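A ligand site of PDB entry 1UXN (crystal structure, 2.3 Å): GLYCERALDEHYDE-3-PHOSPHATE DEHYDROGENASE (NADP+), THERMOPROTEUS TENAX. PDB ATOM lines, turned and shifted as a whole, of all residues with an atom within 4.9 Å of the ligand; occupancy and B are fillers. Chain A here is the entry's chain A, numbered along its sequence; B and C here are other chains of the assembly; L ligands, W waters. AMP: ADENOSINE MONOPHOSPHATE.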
ATOM      1  N   ARG A  72     -25.067 -25.935  34.842  1.00  0.00           N
ATOM      2  CA  ARG A  72     -24.936 -25.874  33.391  1.00  0.00           C
ATOM      3  C   ARG A  72     -25.513 -27.085  32.690  1.00  0.00           C
ATOM      4  O   ARG A  72     -26.161 -26.962  31.640  1.00  0.00           O
ATOM      5  CB  ARG A  72     -23.454 -25.699  33.006  1.00  0.00           C
ATOM      6  CG  ARG A  72     -23.215 -25.426  31.530  1.00  0.00           C
ATOM      7  CD  ARG A  72     -21.759 -25.085  31.242  1.00  0.00           C
ATOM      8  NE  ARG A  72     -21.529 -24.919  29.814  1.00  0.00           N
ATOM      9  CZ  ARG A  72     -20.337 -24.663  29.264  1.00  0.00           C
ATOM     10  NH1 ARG A  72     -19.256 -24.545  30.043  1.00  0.00           N
ATOM     11  NH2 ARG A  72     -20.230 -24.534  27.952  1.00  0.00           N
ATOM     12  N   GLY A  76     -32.133 -25.558  30.455  1.00  0.00           N
ATOM     13  CA  GLY A  76     -32.925 -24.394  30.802  1.00  0.00           C
ATOM     14  C   GLY A  76     -34.393 -24.679  31.149  1.00  0.00           C
ATOM     15  O   GLY A  76     -34.980 -24.048  32.050  1.00  0.00           O
ATOM     16  N   ARG A  79     -34.356 -25.770  34.665  1.00  0.00           N
ATOM     17  CA  ARG A  79     -33.969 -24.697  35.555  1.00  0.00           C
ATOM     18  C   ARG A  79     -35.190 -23.831  35.811  1.00  0.00           C
ATOM     19  O   ARG A  79     -35.453 -23.411  36.924  1.00  0.00           O
ATOM     20  CB  ARG A  79     -32.878 -23.812  34.934  1.00  0.00           C
ATOM     21  CG  ARG A  79     -31.522 -24.459  34.809  1.00  0.00           C
ATOM     22  CD  ARG A  79     -30.504 -23.388  34.385  1.00  0.00           C
ATOM     23  NE  ARG A  79     -29.438 -23.995  33.614  1.00  0.00           N
ATOM     24  CZ  ARG A  79     -29.064 -23.621  32.393  1.00  0.00           C
ATOM     25  NH1 ARG A  79     -29.661 -22.600  31.779  1.00  0.00           N
ATOM     26  NH2 ARG A  79     -28.113 -24.304  31.788  1.00  0.00           N
ATOM     27  N   LYS A 132     -33.288 -11.830  26.291  1.00  0.00           N
ATOM     28  CA  LYS A 132     -31.964 -11.388  25.855  1.00  0.00           C
ATOM     29  C   LYS A 132     -31.039 -12.573  25.603  1.00  0.00           C
ATOM     30  O   LYS A 132     -29.811 -12.490  25.810  1.00  0.00           O
ATOM     31  CB  LYS A 132     -31.324 -10.455  26.887  1.00  0.00           C
ATOM     32  CG  LYS A 132     -32.024  -9.134  27.103  1.00  0.00           C
ATOM     33  CD  LYS A 132     -32.303  -8.408  25.805  1.00  0.00           C
ATOM     34  CE  LYS A 132     -33.001  -7.072  26.084  1.00  0.00           C
ATOM     35  NZ  LYS A 132     -33.784  -6.567  24.896  1.00  0.00           N
ATOM     36  N   ILE A 133     -31.631 -13.697  25.200  1.00  0.00           N
ATOM     37  CA  ILE A 133     -30.841 -14.864  24.861  1.00  0.00           C
ATOM     38  C   ILE A 133     -30.852 -14.871  23.349  1.00  0.00           C
ATOM     39  O   ILE A 133     -31.906 -14.671  22.726  1.00  0.00           O
ATOM     40  CB  ILE A 133     -31.464 -16.189  25.390  1.00  0.00           C
ATOM     41  CG1 ILE A 133     -31.044 -16.411  26.831  1.00  0.00           C
ATOM     42  CG2 ILE A 133     -30.992 -17.380  24.572  1.00  0.00           C
ATOM     43  CD1 ILE A 133     -31.480 -17.755  27.400  1.00  0.00           C
ATOM     44  N   GLY A 134     -29.687 -15.066  22.747  1.00  0.00           N
ATOM     45  CA  GLY A 134     -29.593 -15.089  21.305  1.00  0.00           C
ATOM     46  C   GLY A 134     -28.137 -14.938  20.949  1.00  0.00           C
ATOM     47  O   GLY A 134     -27.274 -15.561  21.558  1.00  0.00           O
ATOM     48  N   GLY A 135     -27.857 -14.123  19.951  1.00  0.00           N
ATOM     49  CA  GLY A 135     -26.483 -13.870  19.582  1.00  0.00           C
ATOM     50  C   GLY A 135     -26.482 -13.271  18.202  1.00  0.00           C
ATOM     51  O   GLY A 135     -27.533 -12.890  17.677  1.00  0.00           O
ATOM     52  N   ARG A 154     -22.084 -15.741  20.928  1.00  0.00           N
ATOM     53  CA  ARG A 154     -23.147 -16.128  21.870  1.00  0.00           C
ATOM     54  C   ARG A 154     -22.651 -15.915  23.284  1.00  0.00           C
ATOM     55  O   ARG A 154     -21.525 -15.450  23.472  1.00  0.00           O
ATOM     56  CB  ARG A 154     -23.565 -17.588  21.667  1.00  0.00           C
ATOM     57  CG  ARG A 154     -22.429 -18.580  21.729  1.00  0.00           C
ATOM     58  CD  ARG A 154     -22.986 -19.971  21.981  1.00  0.00           C
ATOM     59  NE  ARG A 154     -23.233 -20.144  23.402  1.00  0.00           N
ATOM     60  CZ  ARG A 154     -23.950 -21.124  23.929  1.00  0.00           C
ATOM     61  NH1 ARG A 154     -24.507 -22.040  23.136  1.00  0.00           N
ATOM     62  NH2 ARG A 154     -24.096 -21.194  25.250  1.00  0.00           N
ATOM     63  N   ARG A 155     -23.480 -16.214  24.270  1.00  0.00           N
ATOM     64  CA  ARG A 155     -23.063 -16.075  25.667  1.00  0.00           C
ATOM     65  C   ARG A 155     -22.972 -17.406  26.371  1.00  0.00           C
ATOM     66  O   ARG A 155     -23.584 -18.377  25.979  1.00  0.00           O
ATOM     67  CB  ARG A 155     -24.002 -15.176  26.456  1.00  0.00           C
ATOM     68  CG  ARG A 155     -23.941 -13.714  26.048  1.00  0.00           C
ATOM     69  CD  ARG A 155     -24.939 -12.936  26.880  1.00  0.00           C
ATOM     70  NE  ARG A 155     -25.333 -11.685  26.269  1.00  0.00           N
ATOM     71  CZ  ARG A 155     -24.723 -10.524  26.469  1.00  0.00           C
ATOM     72  NH1 ARG A 155     -23.672 -10.446  27.279  1.00  0.00           N
ATOM     73  NH2 ARG A 155     -25.205  -9.432  25.866  1.00  0.00           N
ATOM     74  N   GLU A 156     -22.186 -17.414  27.447  1.00  0.00           N
ATOM     75  CA  GLU A 156     -21.973 -18.590  28.237  1.00  0.00           C
ATOM     76  C   GLU A 156     -21.916 -18.233  29.711  1.00  0.00           C
ATOM     77  O   GLU A 156     -21.453 -17.155  30.079  1.00  0.00           O
ATOM     78  CB  GLU A 156     -20.655 -19.244  27.809  1.00  0.00           C
ATOM     79  CG  GLU A 156     -20.903 -20.650  27.318  1.00  0.00           C
ATOM     80  CD  GLU A 156     -19.692 -21.281  26.700  1.00  0.00           C
ATOM     81  OE1 GLU A 156     -18.582 -21.222  27.322  1.00  0.00           O
ATOM     82  OE2 GLU A 156     -19.875 -21.853  25.594  1.00  0.00           O
ATOM     83  N   PRO A 157     -22.416 -19.127  30.593  1.00  0.00           N
ATOM     84  CA  PRO A 157     -22.355 -18.786  32.015  1.00  0.00           C
ATOM     85  C   PRO A 157     -20.897 -18.756  32.423  1.00  0.00           C
ATOM     86  O   PRO A 157     -20.083 -19.482  31.860  1.00  0.00           O
ATOM     87  CB  PRO A 157     -23.136 -19.930  32.699  1.00  0.00           C
ATOM     88  CG  PRO A 157     -22.989 -21.072  31.749  1.00  0.00           C
ATOM     89  CD  PRO A 157     -23.099 -20.426  30.369  1.00  0.00           C
ATOM     90  N   TYR A 184     -29.134 -18.839  33.655  1.00  0.00           N
ATOM     91  CA  TYR A 184     -28.180 -18.953  32.544  1.00  0.00           C
ATOM     92  C   TYR A 184     -27.163 -20.076  32.722  1.00  0.00           C
ATOM     93  O   TYR A 184     -26.291 -20.270  31.872  1.00  0.00           O
ATOM     94  CB  TYR A 184     -27.453 -17.609  32.315  1.00  0.00           C
ATOM     95  CG  TYR A 184     -28.426 -16.498  32.039  1.00  0.00           C
ATOM     96  CD1 TYR A 184     -29.257 -16.552  30.935  1.00  0.00           C
ATOM     97  CD2 TYR A 184     -28.553 -15.408  32.901  1.00  0.00           C
ATOM     98  CE1 TYR A 184     -30.190 -15.575  30.694  1.00  0.00           C
ATOM     99  CE2 TYR A 184     -29.521 -14.405  32.664  1.00  0.00           C
ATOM    100  CZ  TYR A 184     -30.320 -14.498  31.549  1.00  0.00           C
ATOM    101  OH  TYR A 184     -31.257 -13.515  31.253  1.00  0.00           O
ATOM    102  N   VAL A 479     -28.178 -10.706  32.617  1.00  0.00           N
ATOM    103  CA  VAL A 479     -27.388 -11.714  31.938  1.00  0.00           C
ATOM    104  C   VAL A 479     -25.952 -11.179  31.648  1.00  0.00           C
ATOM    105  O   VAL A 479     -24.972 -11.944  31.639  1.00  0.00           O
ATOM    106  CB  VAL A 479     -28.059 -12.135  30.603  1.00  0.00           C
ATOM    107  CG1 VAL A 479     -27.973 -11.002  29.594  1.00  0.00           C
ATOM    108  CG2 VAL A 479     -27.430 -13.411  30.057  1.00  0.00           C
ATOM    109  N   THR A 483     -22.551 -13.688  32.715  1.00  0.00           N
ATOM    110  CA  THR A 483     -22.297 -14.454  31.515  1.00  0.00           C
ATOM    111  C   THR A 483     -21.135 -13.781  30.728  1.00  0.00           C
ATOM    112  O   THR A 483     -20.854 -12.616  30.943  1.00  0.00           O
ATOM    113  CB  THR A 483     -23.638 -14.497  30.764  1.00  0.00           C
ATOM    114  OG1 THR A 483     -23.876 -15.813  30.273  1.00  0.00           O
ATOM    115  CG2 THR A 483     -23.730 -13.464  29.695  1.00  0.00           C
ATOM    116  N   ARG B 436     -18.306 -28.954  17.269  1.00  0.00           N
ATOM    117  CA  ARG B 436     -19.282 -28.418  18.205  1.00  0.00           C
ATOM    118  C   ARG B 436     -18.923 -28.722  19.651  1.00  0.00           C
ATOM    119  O   ARG B 436     -19.082 -27.868  20.518  1.00  0.00           O
ATOM    120  CB  ARG B 436     -20.688 -28.952  17.951  1.00  0.00           C
ATOM    121  CG  ARG B 436     -21.736 -28.208  18.768  1.00  0.00           C
ATOM    122  CD  ARG B 436     -21.743 -26.726  18.367  1.00  0.00           C
ATOM    123  NE  ARG B 436     -22.675 -25.934  19.162  1.00  0.00           N
ATOM    124  CZ  ARG B 436     -22.424 -25.475  20.386  1.00  0.00           C
ATOM    125  NH1 ARG B 436     -21.268 -25.749  20.972  1.00  0.00           N
ATOM    126  NH2 ARG B 436     -23.309 -24.714  21.007  1.00  0.00           N
ATOM    127  N   ARG B 440     -18.089 -25.924  22.561  1.00  0.00           N
ATOM    128  CA  ARG B 440     -18.782 -25.824  23.841  1.00  0.00           C
ATOM    129  C   ARG B 440     -17.838 -25.909  25.036  1.00  0.00           C
ATOM    130  O   ARG B 440     -17.951 -25.128  25.979  1.00  0.00           O
ATOM    131  CB  ARG B 440     -19.845 -26.922  23.940  1.00  0.00           C
ATOM    132  CG  ARG B 440     -20.459 -27.053  25.318  1.00  0.00           C
ATOM    133  CD  ARG B 440     -21.706 -27.956  25.360  1.00  0.00           C
ATOM    134  NE  ARG B 440     -22.244 -27.841  26.701  1.00  0.00           N
ATOM    135  CZ  ARG B 440     -21.964 -28.650  27.700  1.00  0.00           C
ATOM    136  NH1 ARG B 440     -21.165 -29.696  27.534  1.00  0.00           N
ATOM    137  NH2 ARG B 440     -22.413 -28.341  28.904  1.00  0.00           N
ATOM    138  N   TYR C 137     -28.933 -16.727  17.456  1.00  0.00           N
ATOM    139  CA  TYR C 137     -28.637 -18.060  17.817  1.00  0.00           C
ATOM    140  C   TYR C 137     -29.813 -18.452  18.700  1.00  0.00           C
ATOM    141  O   TYR C 137     -30.253 -17.668  19.568  1.00  0.00           O
ATOM    142  CB  TYR C 137     -27.344 -18.064  18.592  1.00  0.00           C
ATOM    143  CG  TYR C 137     -27.080 -19.355  19.282  1.00  0.00           C
ATOM    144  CD1 TYR C 137     -26.784 -20.506  18.548  1.00  0.00           C
ATOM    145  CD2 TYR C 137     -27.140 -19.452  20.675  1.00  0.00           C
ATOM    146  CE1 TYR C 137     -26.556 -21.716  19.190  1.00  0.00           C
ATOM    147  CE2 TYR C 137     -26.917 -20.653  21.319  1.00  0.00           C
ATOM    148  CZ  TYR C 137     -26.628 -21.784  20.583  1.00  0.00           C
ATOM    149  OH  TYR C 137     -26.410 -22.977  21.231  1.00  0.00           O
ATOM    150  N   PRO C 139     -30.591 -21.355  21.195  1.00  0.00           N
ATOM    151  CA  PRO C 139     -30.148 -22.590  21.868  1.00  0.00           C
ATOM    152  C   PRO C 139     -31.405 -23.447  22.065  1.00  0.00           C
ATOM    153  O   PRO C 139     -32.500 -22.902  22.272  1.00  0.00           O
ATOM    154  CB  PRO C 139     -29.564 -22.077  23.184  1.00  0.00           C
ATOM    155  CG  PRO C 139     -30.426 -20.843  23.461  1.00  0.00           C
ATOM    156  CD  PRO C 139     -30.496 -20.192  22.091  1.00  0.00           C
ATOM    157  N   ASP C 141     -32.198 -25.829  24.555  1.00  0.00           N
ATOM    158  CA  ASP C 141     -32.545 -26.415  25.839  1.00  0.00           C
ATOM    159  C   ASP C 141     -33.681 -25.772  26.635  1.00  0.00           C
ATOM    160  O   ASP C 141     -33.794 -26.028  27.830  1.00  0.00           O
ATOM    161  CB  ASP C 141     -31.309 -26.504  26.731  1.00  0.00           C
ATOM    162  CG  ASP C 141     -30.654 -25.158  26.949  1.00  0.00           C
ATOM    163  OD1 ASP C 141     -30.368 -24.494  25.915  1.00  0.00           O
ATOM    164  OD2 ASP C 141     -30.443 -24.753  28.127  1.00  0.00           O
ATOM    165  N   TRP C 142     -34.508 -24.970  25.983  1.00  0.00           N
ATOM    166  CA  TRP C 142     -35.622 -24.314  26.678  1.00  0.00           C
ATOM    167  C   TRP C 142     -36.938 -25.055  26.468  1.00  0.00           C
ATOM    168  O   TRP C 142     -37.990 -24.620  26.913  1.00  0.00           O
ATOM    169  CB  TRP C 142     -35.722 -22.841  26.231  1.00  0.00           C
ATOM    170  CG  TRP C 142     -34.496 -22.142  26.685  1.00  0.00           C
ATOM    171  CD1 TRP C 142     -33.360 -21.911  25.954  1.00  0.00           C
ATOM    172  CD2 TRP C 142     -34.185 -21.779  28.033  1.00  0.00           C
ATOM    173  NE1 TRP C 142     -32.349 -21.443  26.783  1.00  0.00           N
ATOM    174  CE2 TRP C 142     -32.837 -21.338  28.062  1.00  0.00           C
ATOM    175  CE3 TRP C 142     -34.920 -21.781  29.234  1.00  0.00           C
ATOM    176  CZ2 TRP C 142     -32.203 -20.910  29.224  1.00  0.00           C
ATOM    177  CZ3 TRP C 142     -34.286 -21.354  30.396  1.00  0.00           C
ATOM    178  CH2 TRP C 142     -32.941 -20.923  30.386  1.00  0.00           C
ATOM    179  N   TRP C 498     -23.778 -32.038  24.472  1.00  0.00           N
ATOM    180  CA  TRP C 498     -24.333 -31.722  25.793  1.00  0.00           C
ATOM    181  C   TRP C 498     -24.460 -33.023  26.612  1.00  0.00           C
ATOM    182  O   TRP C 498     -24.473 -34.121  26.056  1.00  0.00           O
ATOM    183  CB  TRP C 498     -25.713 -31.058  25.639  1.00  0.00           C
ATOM    184  CG  TRP C 498     -25.599 -29.665  25.107  1.00  0.00           C
ATOM    185  CD1 TRP C 498     -25.193 -28.555  25.794  1.00  0.00           C
ATOM    186  CD2 TRP C 498     -25.787 -29.253  23.758  1.00  0.00           C
ATOM    187  NE1 TRP C 498     -25.100 -27.492  24.955  1.00  0.00           N
ATOM    188  CE2 TRP C 498     -25.454 -27.883  23.687  1.00  0.00           C
ATOM    189  CE3 TRP C 498     -26.194 -29.909  22.578  1.00  0.00           C
ATOM    190  CZ2 TRP C 498     -25.518 -27.138  22.497  1.00  0.00           C
ATOM    191  CZ3 TRP C 498     -26.265 -29.181  21.391  1.00  0.00           C
ATOM    192  CH2 TRP C 498     -25.928 -27.800  21.359  1.00  0.00           C
HETATM  193  P   AMP L   1     -23.825 -24.553  26.862  1.00  0.00           P
HETATM  194  O1P AMP L   1     -23.602 -25.854  27.550  1.00  0.00           O
HETATM  195  O2P AMP L   1     -24.479 -24.572  25.564  1.00  0.00           O
HETATM  196  O3P AMP L   1     -22.539 -23.727  26.826  1.00  0.00           O
HETATM  197  O5' AMP L   1     -24.809 -23.843  27.901  1.00  0.00           O
HETATM  198  C5' AMP L   1     -25.190 -22.528  27.660  1.00  0.00           C
HETATM  199  C4' AMP L   1     -26.396 -22.218  28.510  1.00  0.00           C
HETATM  200  O4' AMP L   1     -26.577 -20.816  28.137  1.00  0.00           O
HETATM  201  C3' AMP L   1     -27.765 -23.026  27.976  1.00  0.00           C
HETATM  202  O3' AMP L   1     -28.718 -23.028  29.145  1.00  0.00           O
HETATM  203  C2' AMP L   1     -28.168 -22.027  26.828  1.00  0.00           C
HETATM  204  O2' AMP L   1     -29.508 -22.015  26.486  1.00  0.00           O
HETATM  205  C1' AMP L   1     -27.777 -20.611  27.442  1.00  0.00           C
HETATM  206  N9  AMP L   1     -27.479 -19.600  26.429  1.00  0.00           N
HETATM  207  C8  AMP L   1     -27.155 -19.768  25.076  1.00  0.00           C
HETATM  208  N7  AMP L   1     -26.940 -18.650  24.367  1.00  0.00           N
HETATM  209  C5  AMP L   1     -27.162 -17.710  25.364  1.00  0.00           C
HETATM  210  C6  AMP L   1     -27.124 -16.300  25.331  1.00  0.00           C
HETATM  211  N6  AMP L   1     -26.819 -15.678  24.146  1.00  0.00           N
HETATM  212  N1  AMP L   1     -27.405 -15.652  26.549  1.00  0.00           N
HETATM  213  C2  AMP L   1     -27.699 -16.311  27.685  1.00  0.00           C
HETATM  214  N3  AMP L   1     -27.763 -17.660  27.809  1.00  0.00           N
HETATM  215  C4  AMP L   1     -27.495 -18.279  26.624  1.00  0.00           C
HETATM  216  O   HOH W   1     -26.380 -23.447  23.950  1.00  0.00           O
HETATM  217  O   HOH W   2     -27.501 -12.725  24.149  1.00  0.00           O
HETATM  218  O   HOH W   3     -21.976 -24.160  23.764  1.00  0.00           O
HETATM  219  O   HOH W   4     -26.056 -26.491  28.724  1.00  0.00           O
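An oxygen (O1P) of the ligand lies within salt-bridge range of the guanidinium group (NE) of Arg 440 of chain B, at 2.6 Å. The backbone carbonyl oxygen (O) of Gly 134 is in hydrogen-bond range of a nitrogen (N6) of the ligand, at 2.6 Å. OD2 of Asp 141 of chain C is in hydrogen-bond range of O3' of the ligand (2.6 Å). O3P of the ligand is in salt-bridge range of NH2 of Arg 72, 2.7 Å away. The guanidinium group (NH1) of Arg 79 sits at hydrogen-bond distance from an oxygen (O3') of the ligand (2.8 Å). NE1 of Trp 142 of chain C is in hydrogen-bond range of O2' of the ligand (2.9 Å). The guanidinium group (NH2) of Arg 154 lies within salt-bridge range of an oxygen (O3P) of the ligand (3.4 Å). NE1 of Trp 498 of chain C lies within hydrogen-bond range of O2P of the ligand (3.0 Å).
The backbone carbonyl oxygen of Arg 440 of chain B is in hydrogen-bond range of the guanidinium group of Arg 72, 3.1 Å away. The side-chain carboxylate (OD2) of Asp 141 of chain C sits at hydrogen-bond distance from the backbone NH (N) of Gly 76 (3.0 Å). O of Arg 72 is in hydrogen-bond range of NH2 of Arg 79 (3.3 Å). OE2 of Glu 156 is in salt-bridge range of NH2 of Arg 72 (3.6 Å). NH1 of Arg 154 sits at hydrogen-bond distance from OH of Tyr 137 of chain C. The backbone carbonyl oxygen of Glu 156 sits at hydrogen-bond distance from the side-chain hydroxyl of Thr 483 (2.8 Å).
A nitrogen (N6) of the ligand sits close to the backbone NH of Arg 155 (3.4 Å). OE2 of Glu 156 sits close to O3P of the ligand (3.5 Å). Residues that only touch the ligand: Pro 139 of chain C, Ile 133, Tyr 184, Tyr 137 of chain C and Val 479. Hydrophobic or aromatic side chains within 4 Å of the ligand: Ile 133, Tyr 184, Val 479, Tyr 137 of chain C, Pro 139 of chain C, Trp 142 of chain C and Trp 498 of chain C. 15 residues have an atom within 4 Å of the ligand: Arg 72, Arg 79, Ile 133, Gly 134, Arg 154, Arg 155, Glu 156, Tyr 184, Val 479, Arg 440 of chain B, Tyr 137 of chain C, Pro 139 of chain C, Asp 141 of chain C, Trp 142 of chain C and Trp 498 of chain C. Along chain A the residues within 4 Å of the ligand span positions 72 to 479. The nearest printed residue that does not touch the ligand is Pro 157 (4.02 Å).
Water W1 lies within hydrogen-bond range of the guanidinium group of Arg 154 (2.5 Å), an oxygen (O2P) of the ligand (2.7 Å) and the side-chain hydroxyl of Tyr 137 of chain C (2.8 Å). Water W4 bridges O1P of the ligand and O of Arg 72. Water W3 lies within hydrogen-bond range of an oxygen (O2P) of the ligand, the guanidinium group (NH2) of Arg 436 of chain B and the guanidinium group (NH1) of Arg 154.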
